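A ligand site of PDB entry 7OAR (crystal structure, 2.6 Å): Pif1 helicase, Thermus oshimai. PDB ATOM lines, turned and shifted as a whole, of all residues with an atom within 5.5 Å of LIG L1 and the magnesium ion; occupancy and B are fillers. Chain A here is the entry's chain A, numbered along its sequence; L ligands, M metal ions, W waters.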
ATOM      1  N   GLU A   7      -9.760  20.244 -33.893  1.00  0.00           N
ATOM      2  CA  GLU A   7     -10.183  19.849 -35.225  1.00  0.00           C
ATOM      3  C   GLU A   7      -9.429  20.566 -36.326  1.00  0.00           C
ATOM      4  O   GLU A   7      -9.979  21.518 -36.869  1.00  0.00           O
ATOM      5  CB  GLU A   7     -11.676  20.140 -35.465  1.00  0.00           C
ATOM      6  CG  GLU A   7     -12.627  19.877 -34.342  1.00  0.00           C
ATOM      7  CD  GLU A   7     -12.300  18.637 -33.548  1.00  0.00           C
ATOM      8  OE1 GLU A   7     -11.576  18.747 -32.543  1.00  0.00           O
ATOM      9  OE2 GLU A   7     -12.798  17.564 -33.927  1.00  0.00           O
ATOM     10  N   GLY A   8      -8.234  20.124 -36.719  1.00  0.00           N
ATOM     11  CA  GLY A   8      -7.869  20.681 -38.005  1.00  0.00           C
ATOM     12  C   GLY A   8      -6.701  21.621 -38.197  1.00  0.00           C
ATOM     13  O   GLY A   8      -6.818  22.490 -39.066  1.00  0.00           O
ATOM     14  N   LEU A   9      -5.621  21.509 -37.430  1.00  0.00           N
ATOM     15  CA  LEU A   9      -4.875  22.659 -36.914  1.00  0.00           C
ATOM     16  C   LEU A   9      -4.781  23.799 -37.906  1.00  0.00           C
ATOM     17  O   LEU A   9      -4.416  23.606 -39.069  1.00  0.00           O
ATOM     18  CB  LEU A   9      -3.456  22.233 -36.496  1.00  0.00           C
ATOM     19  CG  LEU A   9      -3.170  21.154 -35.450  1.00  0.00           C
ATOM     20  CD1 LEU A   9      -3.873  21.463 -34.141  1.00  0.00           C
ATOM     21  CD2 LEU A   9      -3.509  19.734 -35.947  1.00  0.00           C
ATOM     22  N   SER A  10      -5.144  24.992 -37.436  1.00  0.00           N
ATOM     23  CA  SER A  10      -5.042  26.222 -38.185  1.00  0.00           C
ATOM     24  C   SER A  10      -3.577  26.536 -38.475  1.00  0.00           C
ATOM     25  O   SER A  10      -2.649  25.934 -37.920  1.00  0.00           O
ATOM     26  CB  SER A  10      -5.651  27.366 -37.392  1.00  0.00           C
ATOM     27  OG  SER A  10      -4.634  28.060 -36.674  1.00  0.00           O
ATOM     28  N   GLN A  13      -2.024  27.612 -35.401  1.00  0.00           N
ATOM     29  CA  GLN A  13      -1.909  26.503 -34.465  1.00  0.00           C
ATOM     30  C   GLN A  13      -0.717  25.628 -34.802  1.00  0.00           C
ATOM     31  O   GLN A  13       0.105  25.315 -33.928  1.00  0.00           O
ATOM     32  CB  GLN A  13      -3.187  25.680 -34.454  1.00  0.00           C
ATOM     33  CG  GLN A  13      -4.222  26.178 -33.490  1.00  0.00           C
ATOM     34  CD  GLN A  13      -5.537  25.492 -33.717  1.00  0.00           C
ATOM     35  OE1 GLN A  13      -5.920  25.226 -34.860  1.00  0.00           O
ATOM     36  NE2 GLN A  13      -6.244  25.188 -32.634  1.00  0.00           N
ATOM     37  N   PRO A  33      -6.672  34.792 -26.743  1.00  0.00           N
ATOM     38  CA  PRO A  33      -8.059  35.020 -26.310  1.00  0.00           C
ATOM     39  C   PRO A  33      -8.836  33.714 -26.193  1.00  0.00           C
ATOM     40  O   PRO A  33      -8.414  32.635 -26.641  1.00  0.00           O
ATOM     41  CB  PRO A  33      -8.647  35.901 -27.416  1.00  0.00           C
ATOM     42  CG  PRO A  33      -7.465  36.557 -28.025  1.00  0.00           C
ATOM     43  CD  PRO A  33      -6.320  35.614 -27.909  1.00  0.00           C
ATOM     44  N   ALA A  34     -10.010  33.822 -25.572  1.00  0.00           N
ATOM     45  CA  ALA A  34     -10.865  32.656 -25.401  1.00  0.00           C
ATOM     46  C   ALA A  34     -11.250  32.053 -26.763  1.00  0.00           C
ATOM     47  O   ALA A  34     -11.513  32.768 -27.727  1.00  0.00           O
ATOM     48  CB  ALA A  34     -12.108  33.054 -24.625  1.00  0.00           C
ATOM     49  N   GLY A  35     -11.232  30.722 -26.838  1.00  0.00           N
ATOM     50  CA  GLY A  35     -11.696  30.029 -28.023  1.00  0.00           C
ATOM     51  C   GLY A  35     -10.740  29.977 -29.200  1.00  0.00           C
ATOM     52  O   GLY A  35     -11.179  29.652 -30.304  1.00  0.00           O
ATOM     53  N   THR A  36      -9.469  30.290 -28.999  1.00  0.00           N
ATOM     54  CA  THR A  36      -8.504  30.301 -30.095  1.00  0.00           C
ATOM     55  C   THR A  36      -8.007  28.913 -30.471  1.00  0.00           C
ATOM     56  O   THR A  36      -7.300  28.774 -31.489  1.00  0.00           O
ATOM     57  CB  THR A  36      -7.294  31.166 -29.707  1.00  0.00           C
ATOM     58  OG1 THR A  36      -7.756  32.254 -28.894  1.00  0.00           O
ATOM     59  CG2 THR A  36      -6.689  31.759 -30.942  1.00  0.00           C
ATOM     60  N   GLY A  37      -8.353  27.896 -29.705  1.00  0.00           N
ATOM     61  CA  GLY A  37      -7.919  26.544 -29.952  1.00  0.00           C
ATOM     62  C   GLY A  37      -6.730  26.130 -29.126  1.00  0.00           C
ATOM     63  O   GLY A  37      -5.990  25.238 -29.555  1.00  0.00           O
ATOM     64  N   LYS A  38      -6.504  26.752 -27.977  1.00  0.00           N
ATOM     65  CA  LYS A  38      -5.362  26.348 -27.168  1.00  0.00           C
ATOM     66  C   LYS A  38      -5.492  24.896 -26.750  1.00  0.00           C
ATOM     67  O   LYS A  38      -4.569  24.086 -26.980  1.00  0.00           O
ATOM     68  CB  LYS A  38      -5.220  27.276 -25.959  1.00  0.00           C
ATOM     69  CG  LYS A  38      -4.972  28.725 -26.353  1.00  0.00           C
ATOM     70  CD  LYS A  38      -4.840  29.662 -25.141  1.00  0.00           C
ATOM     71  CE  LYS A  38      -6.174  29.919 -24.462  1.00  0.00           C
ATOM     72  NZ  LYS A  38      -7.223  30.523 -25.315  1.00  0.00           N
ATOM     73  N   THR A  39      -6.653  24.514 -26.220  1.00  0.00           N
ATOM     74  CA  THR A  39      -6.821  23.133 -25.764  1.00  0.00           C
ATOM     75  C   THR A  39      -6.809  22.153 -26.941  1.00  0.00           C
ATOM     76  O   THR A  39      -6.299  21.039 -26.821  1.00  0.00           O
ATOM     77  CB  THR A  39      -8.112  23.012 -24.960  1.00  0.00           C
ATOM     78  OG1 THR A  39      -8.065  23.923 -23.860  1.00  0.00           O
ATOM     79  CG2 THR A  39      -8.290  21.591 -24.447  1.00  0.00           C
ATOM     80  N   THR A  40      -7.312  22.579 -28.088  1.00  0.00           N
ATOM     81  CA  THR A  40      -7.254  21.729 -29.274  1.00  0.00           C
ATOM     82  C   THR A  40      -5.810  21.533 -29.722  1.00  0.00           C
ATOM     83  O   THR A  40      -5.423  20.425 -30.126  1.00  0.00           O
ATOM     84  CB  THR A  40      -8.108  22.361 -30.391  1.00  0.00           C
ATOM     85  OG1 THR A  40      -9.488  22.383 -29.997  1.00  0.00           O
ATOM     86  CG2 THR A  40      -7.969  21.577 -31.682  1.00  0.00           C
ATOM     87  N   LEU A  41      -4.983  22.568 -29.594  1.00  0.00           N
ATOM     88  CA  LEU A  41      -3.557  22.384 -29.859  1.00  0.00           C
ATOM     89  C   LEU A  41      -2.945  21.462 -28.807  1.00  0.00           C
ATOM     90  O   LEU A  41      -2.044  20.669 -29.119  1.00  0.00           O
ATOM     91  CB  LEU A  41      -2.846  23.737 -29.857  1.00  0.00           C
ATOM     92  CG  LEU A  41      -1.308  23.830 -29.886  1.00  0.00           C
ATOM     93  CD1 LEU A  41      -0.710  22.945 -30.961  1.00  0.00           C
ATOM     94  CD2 LEU A  41      -0.821  25.265 -30.057  1.00  0.00           C
ATOM     95  N   GLN A  65     -11.498  18.611 -19.904  1.00  0.00           N
ATOM     96  CA  GLN A  65     -11.407  19.144 -21.258  1.00  0.00           C
ATOM     97  C   GLN A  65     -10.051  18.838 -21.879  1.00  0.00           C
ATOM     98  O   GLN A  65      -9.941  18.604 -23.093  1.00  0.00           O
ATOM     99  CB  GLN A  65     -11.649  20.649 -21.261  1.00  0.00           C
ATOM    100  CG  GLN A  65     -13.083  21.051 -21.504  1.00  0.00           C
ATOM    101  CD  GLN A  65     -13.518  20.971 -22.955  1.00  0.00           C
ATOM    102  OE1 GLN A  65     -12.706  21.089 -23.879  1.00  0.00           O
ATOM    103  NE2 GLN A  65     -14.820  20.805 -23.164  1.00  0.00           N
ATOM    104  N   ASP A 112      -2.777  23.056 -18.681  1.00  0.00           N
ATOM    105  CA  ASP A 112      -3.779  23.843 -19.363  1.00  0.00           C
ATOM    106  C   ASP A 112      -4.511  24.727 -18.376  1.00  0.00           C
ATOM    107  O   ASP A 112      -4.532  24.469 -17.171  1.00  0.00           O
ATOM    108  CB  ASP A 112      -4.790  22.951 -20.112  1.00  0.00           C
ATOM    109  CG  ASP A 112      -5.527  23.697 -21.224  1.00  0.00           C
ATOM    110  OD1 ASP A 112      -5.161  24.875 -21.505  1.00  0.00           O
ATOM    111  OD2 ASP A 112      -6.462  23.125 -21.819  1.00  0.00           O
ATOM    112  N   GLU A 113      -5.161  25.755 -18.921  1.00  0.00           N
ATOM    113  CA  GLU A 113      -5.761  26.835 -18.150  1.00  0.00           C
ATOM    114  C   GLU A 113      -4.870  27.259 -16.984  1.00  0.00           C
ATOM    115  O   GLU A 113      -5.297  27.382 -15.825  1.00  0.00           O
ATOM    116  CB  GLU A 113      -7.173  26.451 -17.715  1.00  0.00           C
ATOM    117  CG  GLU A 113      -8.061  26.260 -18.957  1.00  0.00           C
ATOM    118  CD  GLU A 113      -8.695  27.571 -19.470  1.00  0.00           C
ATOM    119  OE1 GLU A 113      -9.908  27.738 -19.285  1.00  0.00           O
ATOM    120  OE2 GLU A 113      -7.982  28.438 -20.022  1.00  0.00           O
ATOM    121  N   GLN A 196     -11.356  30.382 -32.980  1.00  0.00           N
ATOM    122  CA  GLN A 196     -11.954  29.187 -33.564  1.00  0.00           C
ATOM    123  C   GLN A 196     -13.308  28.827 -32.967  1.00  0.00           C
ATOM    124  O   GLN A 196     -14.061  28.083 -33.611  1.00  0.00           O
ATOM    125  CB  GLN A 196     -11.028  27.971 -33.379  1.00  0.00           C
ATOM    126  CG  GLN A 196      -9.611  28.192 -33.836  1.00  0.00           C
ATOM    127  CD  GLN A 196      -9.520  28.361 -35.320  1.00  0.00           C
ATOM    128  OE1 GLN A 196     -10.422  27.930 -36.052  1.00  0.00           O
ATOM    129  NE2 GLN A 196      -8.440  28.985 -35.777  1.00  0.00           N
ATOM    130  N   ARG A 197     -13.647  29.322 -31.774  1.00  0.00           N
ATOM    131  CA  ARG A 197     -14.982  29.052 -31.235  1.00  0.00           C
ATOM    132  C   ARG A 197     -16.044  29.834 -31.990  1.00  0.00           C
ATOM    133  O   ARG A 197     -17.055  29.271 -32.409  1.00  0.00           O
ATOM    134  CB  ARG A 197     -15.050  29.357 -29.745  1.00  0.00           C
ATOM    135  CG  ARG A 197     -16.360  28.894 -29.083  1.00  0.00           C
ATOM    136  CD  ARG A 197     -16.266  28.833 -27.549  1.00  0.00           C
ATOM    137  NE  ARG A 197     -15.238  27.883 -27.095  1.00  0.00           N
ATOM    138  CZ  ARG A 197     -14.335  28.171 -26.153  1.00  0.00           C
ATOM    139  NH1 ARG A 197     -14.339  29.377 -25.579  1.00  0.00           N
ATOM    140  NH2 ARG A 197     -13.417  27.268 -25.796  1.00  0.00           N
ATOM    141  N   ARG A 199     -15.653  31.322 -34.956  1.00  0.00           N
ATOM    142  CA  ARG A 199     -15.100  31.480 -36.298  1.00  0.00           C
ATOM    143  C   ARG A 199     -16.150  31.926 -37.297  1.00  0.00           C
ATOM    144  O   ARG A 199     -15.885  32.757 -38.172  1.00  0.00           O
ATOM    145  CB  ARG A 199     -14.477  30.159 -36.747  1.00  0.00           C
ATOM    146  CG  ARG A 199     -15.493  29.011 -36.854  1.00  0.00           C
ATOM    147  CD  ARG A 199     -14.919  27.655 -36.471  1.00  0.00           C
ATOM    148  NE  ARG A 199     -13.575  27.468 -36.997  1.00  0.00           N
ATOM    149  CZ  ARG A 199     -13.319  27.118 -38.259  1.00  0.00           C
ATOM    150  NH1 ARG A 199     -14.316  26.921 -39.110  1.00  0.00           N
ATOM    151  NH2 ARG A 199     -12.061  26.968 -38.660  1.00  0.00           N
ATOM    152  N   GLY A 377     -13.187  26.793 -19.905  1.00  0.00           N
ATOM    153  CA  GLY A 377     -12.634  25.722 -20.716  1.00  0.00           C
ATOM    154  C   GLY A 377     -13.624  25.138 -21.703  1.00  0.00           C
ATOM    155  O   GLY A 377     -13.235  24.694 -22.787  1.00  0.00           O
ATOM    156  N   THR A 379     -16.782  24.727 -24.432  1.00  0.00           N
ATOM    157  CA  THR A 379     -17.572  25.376 -25.473  1.00  0.00           C
ATOM    158  C   THR A 379     -19.016  24.974 -25.224  1.00  0.00           C
ATOM    159  O   THR A 379     -19.300  23.780 -25.021  1.00  0.00           O
ATOM    160  CB  THR A 379     -17.104  24.972 -26.889  1.00  0.00           C
ATOM    161  OG1 THR A 379     -15.785  25.460 -27.153  1.00  0.00           O
ATOM    162  CG2 THR A 379     -18.019  25.537 -27.962  1.00  0.00           C
ATOM    163  N   ARG A 403     -18.177  31.648 -24.059  1.00  0.00           N
ATOM    164  CA  ARG A 403     -18.363  30.206 -24.105  1.00  0.00           C
ATOM    165  C   ARG A 403     -19.061  29.726 -25.388  1.00  0.00           C
ATOM    166  O   ARG A 403     -18.913  28.559 -25.746  1.00  0.00           O
ATOM    167  CB  ARG A 403     -19.141  29.747 -22.867  1.00  0.00           C
ATOM    168  CG  ARG A 403     -18.451  30.038 -21.534  1.00  0.00           C
ATOM    169  CD  ARG A 403     -17.094  29.355 -21.411  1.00  0.00           C
ATOM    170  NE  ARG A 403     -16.004  30.259 -21.784  1.00  0.00           N
ATOM    171  CZ  ARG A 403     -14.780  29.882 -22.134  1.00  0.00           C
ATOM    172  NH1 ARG A 403     -14.451  28.600 -22.169  1.00  0.00           N
ATOM    173  NH2 ARG A 403     -13.880  30.795 -22.455  1.00  0.00           N
ATOM    174  N   ARG A 405     -20.486  29.915 -29.630  1.00  0.00           N
ATOM    175  CA  ARG A 405     -19.996  30.146 -30.977  1.00  0.00           C
ATOM    176  C   ARG A 405     -20.634  31.363 -31.650  1.00  0.00           C
ATOM    177  O   ARG A 405     -20.014  31.949 -32.549  1.00  0.00           O
ATOM    178  CB  ARG A 405     -20.218  28.898 -31.844  1.00  0.00           C
ATOM    179  CG  ARG A 405     -19.704  27.614 -31.217  1.00  0.00           C
ATOM    180  CD  ARG A 405     -20.251  26.374 -31.912  1.00  0.00           C
ATOM    181  NE  ARG A 405     -19.670  25.163 -31.333  1.00  0.00           N
ATOM    182  CZ  ARG A 405     -20.304  24.341 -30.503  1.00  0.00           C
ATOM    183  NH1 ARG A 405     -21.569  24.593 -30.149  1.00  0.00           N
ATOM    184  NH2 ARG A 405     -19.683  23.275 -30.025  1.00  0.00           N
HETATM  185  P1  LIG L   1      -9.306  27.369 -26.139  1.00  0.00           P
HETATM  186  O1  LIG L   1      -8.382  28.406 -26.754  1.00  0.00           O
HETATM  187  O2  LIG L   1      -8.581  26.242 -25.447  1.00  0.00           O
HETATM  188  O3  LIG L   1     -10.510  27.903 -25.352  1.00  0.00           O
HETATM  189  P2  LIG L   1     -10.598  25.277 -27.648  1.00  0.00           P
HETATM  190  O4  LIG L   1      -9.522  24.300 -28.052  1.00  0.00           O
HETATM  191  O5  LIG L   1     -11.561  25.039 -26.482  1.00  0.00           O
HETATM  192  O6  LIG L   1      -9.876  26.723 -27.499  1.00  0.00           O
HETATM  193  O7  LIG L   1     -11.552  25.593 -28.915  1.00  0.00           O
HETATM  194  C1  LIG L   1     -12.960  25.784 -28.704  1.00  0.00           C
HETATM  195  C2  LIG L   1     -13.741  25.272 -29.897  1.00  0.00           C
HETATM  196  O8  LIG L   1     -13.018  25.644 -31.073  1.00  0.00           O
HETATM  197  C3  LIG L   1     -13.781  23.755 -29.869  1.00  0.00           C
HETATM  198  O9  LIG L   1     -15.129  23.283 -29.885  1.00  0.00           O
HETATM  199  C4  LIG L   1     -13.028  23.292 -31.095  1.00  0.00           C
HETATM  200  O10 LIG L   1     -13.733  22.268 -31.799  1.00  0.00           O
HETATM  201  C5  LIG L   1     -12.940  24.533 -31.948  1.00  0.00           C
HETATM  202  N1  LIG L   1     -11.637  24.569 -32.612  1.00  0.00           N
HETATM  203  C6  LIG L   1     -10.446  24.821 -32.048  1.00  0.00           C
HETATM  204  N2  LIG L   1      -9.456  24.788 -32.973  1.00  0.00           N
HETATM  205  C7  LIG L   1     -10.032  24.498 -34.156  1.00  0.00           C
HETATM  206  C8  LIG L   1      -9.586  24.300 -35.550  1.00  0.00           C
HETATM  207  N3  LIG L   1      -8.267  24.404 -35.889  1.00  0.00           N
HETATM  208  N4  LIG L   1     -10.543  24.023 -36.472  1.00  0.00           N
HETATM  209  C9  LIG L   1     -11.845  23.903 -36.156  1.00  0.00           C
HETATM  210  N5  LIG L   1     -12.322  24.062 -34.918  1.00  0.00           N
HETATM  211  C10 LIG L   1     -11.477  24.359 -33.903  1.00  0.00           C
HETATM  212 AL1  LG2 L   2     -10.640  28.687 -23.404  1.00  0.00          AL
HETATM  213  F1  LG2 L   2     -11.806  29.998 -23.697  1.00  0.00           F
HETATM  214  F2  LG2 L   2      -9.527  27.374 -22.987  1.00  0.00           F
HETATM  215  F3  LG2 L   2      -9.272  29.802 -23.705  1.00  0.00           F
HETATM  216  F4  LG2 L   2     -11.973  27.520 -23.329  1.00  0.00           F
HETATM  217 MG    MG M   1      -8.928  25.594 -23.337  1.00  0.00          MG
HETATM  218  O   HOH W   1      -9.362  25.221 -21.468  1.00  0.00           O
HETATM  219  O   HOH W   2      -6.849  26.332 -23.018  1.00  0.00           O
HETATM  220  O   HOH W   3     -10.675  24.500 -23.656  1.00  0.00           O
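The backbone NH (N) of Gln 196 sits at hydrogen-bond distance from the backbone carbonyl oxygen (O) of Gly 35 (2.8 Å).
N of Ser 10 lies within hydrogen-bond range of OE1 of Gln 13 (2.7 Å).
The side-chain amide nitrogen (NE2) of Gln 13 is in hydrogen-bond range of the backbone carbonyl oxygen (O) of Gly 37.
OE1 of Gln 196 is in hydrogen-bond range of NH2 of Arg 199 (3.2 Å).
The backbone NH (N) of Arg 197 sits at hydrogen-bond distance from the backbone carbonyl oxygen (O) of Gly 35 (2.9 Å).
The side-chain amino group (NZ) of Lys 38 is in hydrogen-bond range of the backbone carbonyl oxygen (O) of Pro 33 (2.8 Å).
The guanidinium group (NE) of Arg 197 lies within hydrogen-bond range of the side-chain hydroxyl (OG1) of Thr 379 (2.5 Å).
The side-chain carboxylate of Asp 112 lies close to the side-chain hydroxyl of Thr 39.
Water W3 lies within hydrogen-bond range of O of Gly 377 (2.7 Å) and O5 of LIG L1 (3.0 Å).
The magnesium ion is bound by a fluorine (F2) of LG2 L2 (1.9 Å), the side-chain hydroxyl of Thr 39 (2.0 Å), water W1 (2.0 Å), water W3 (2.1 Å), water W2 (2.2 Å) and an oxygen (O2) of LIG L1 (2.2 Å).
The magnesium ion has six donor atoms within binding distance.
The side-chain amide oxygen (OE1) of Gln 13 lies within hydrogen-bond range of a nitrogen (N3) of LIG L1 (2.7 Å).
An oxygen (O1) of LIG L1 lies within salt-bridge range of the side-chain amino group (NZ) of Lys 38, at 2.8 Å.
N of Gly 35 sits close to O3 of LIG L1.
An oxygen (O5) of LIG L1 lies within salt-bridge range of the guanidinium group (NH2) of Arg 197, 3.0 Å away.
O of Glu 7 sits close to N3 of LIG L1 (3.5 Å).
An oxygen (O6) of LIG L1 is in hydrogen-bond range of the backbone NH (N) of Gly 37 (2.9 Å).
N of Thr 39 is in hydrogen-bond range of O4 of LIG L1 (3.4 Å).
An oxygen (O1) of LIG L1 lies within hydrogen-bond range of the backbone NH (N) of Thr 36 (3.1 Å).
An oxygen (O4) of LIG L1 is in hydrogen-bond range of the side-chain hydroxyl of Thr 40 (2.7 Å).
An oxygen (O4) of LIG L1 sits at hydrogen-bond distance from the backbone NH (N) of Thr 40 (2.8 Å).
A fluorine (F1) of LG2 L2 sits at hydrogen-bond distance from the backbone NH of Gly 35, 3.3 Å away.
The backbone NH (N) of Lys 38 lies within hydrogen-bond range of an oxygen (O1) of LIG L1, 2.8 Å away.
A fluorine (F1) of LG2 L2 sits at hydrogen-bond distance from the guanidinium group (NH2) of Arg 403 (2.5 Å).
A fluorine (F4) of LG2 L2 lies within hydrogen-bond range of the guanidinium group (NH2) of Arg 197, at 2.9 Å.
A fluorine (F3) of LG2 L2 lies within hydrogen-bond range of the side-chain amino group of Lys 38 (2.7 Å).
C of Gly 8 touches N3 of LIG L1, at 3.9 Å.
Leu 9 touches LIG L1.
Ser 10 touches LIG L1 (N to N3, 3.5 Å).
CB of Gln 196 touches C6 of LIG L1, at 3.5 Å.
Arg 199 touches LIG L1.
Thr 379 touches LIG L1 (OG1 to C1, 3.2 Å).
15 residues have an atom within 4 Å of LIG L1: Glu 7, Gly 8, Leu 9, Ser 10, Gln 13, Gly 35, Thr 36, Gly 37, Lys 38, Thr 39, Thr 40, Gln 196, Arg 197, Arg 199 and Thr 379.
Merely in contact with the magnesium ion: Asp 112 (3.8 Å).
Within 4 Å of the magnesium ion: Thr 39 and Asp 112.
The nearest printed residue that does not touch the magnesium ion is Glu 113 (4.3 Å).
An aluminium atom (AL1) of LG2 L2 is bound by an oxygen (O3) of LIG L1.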
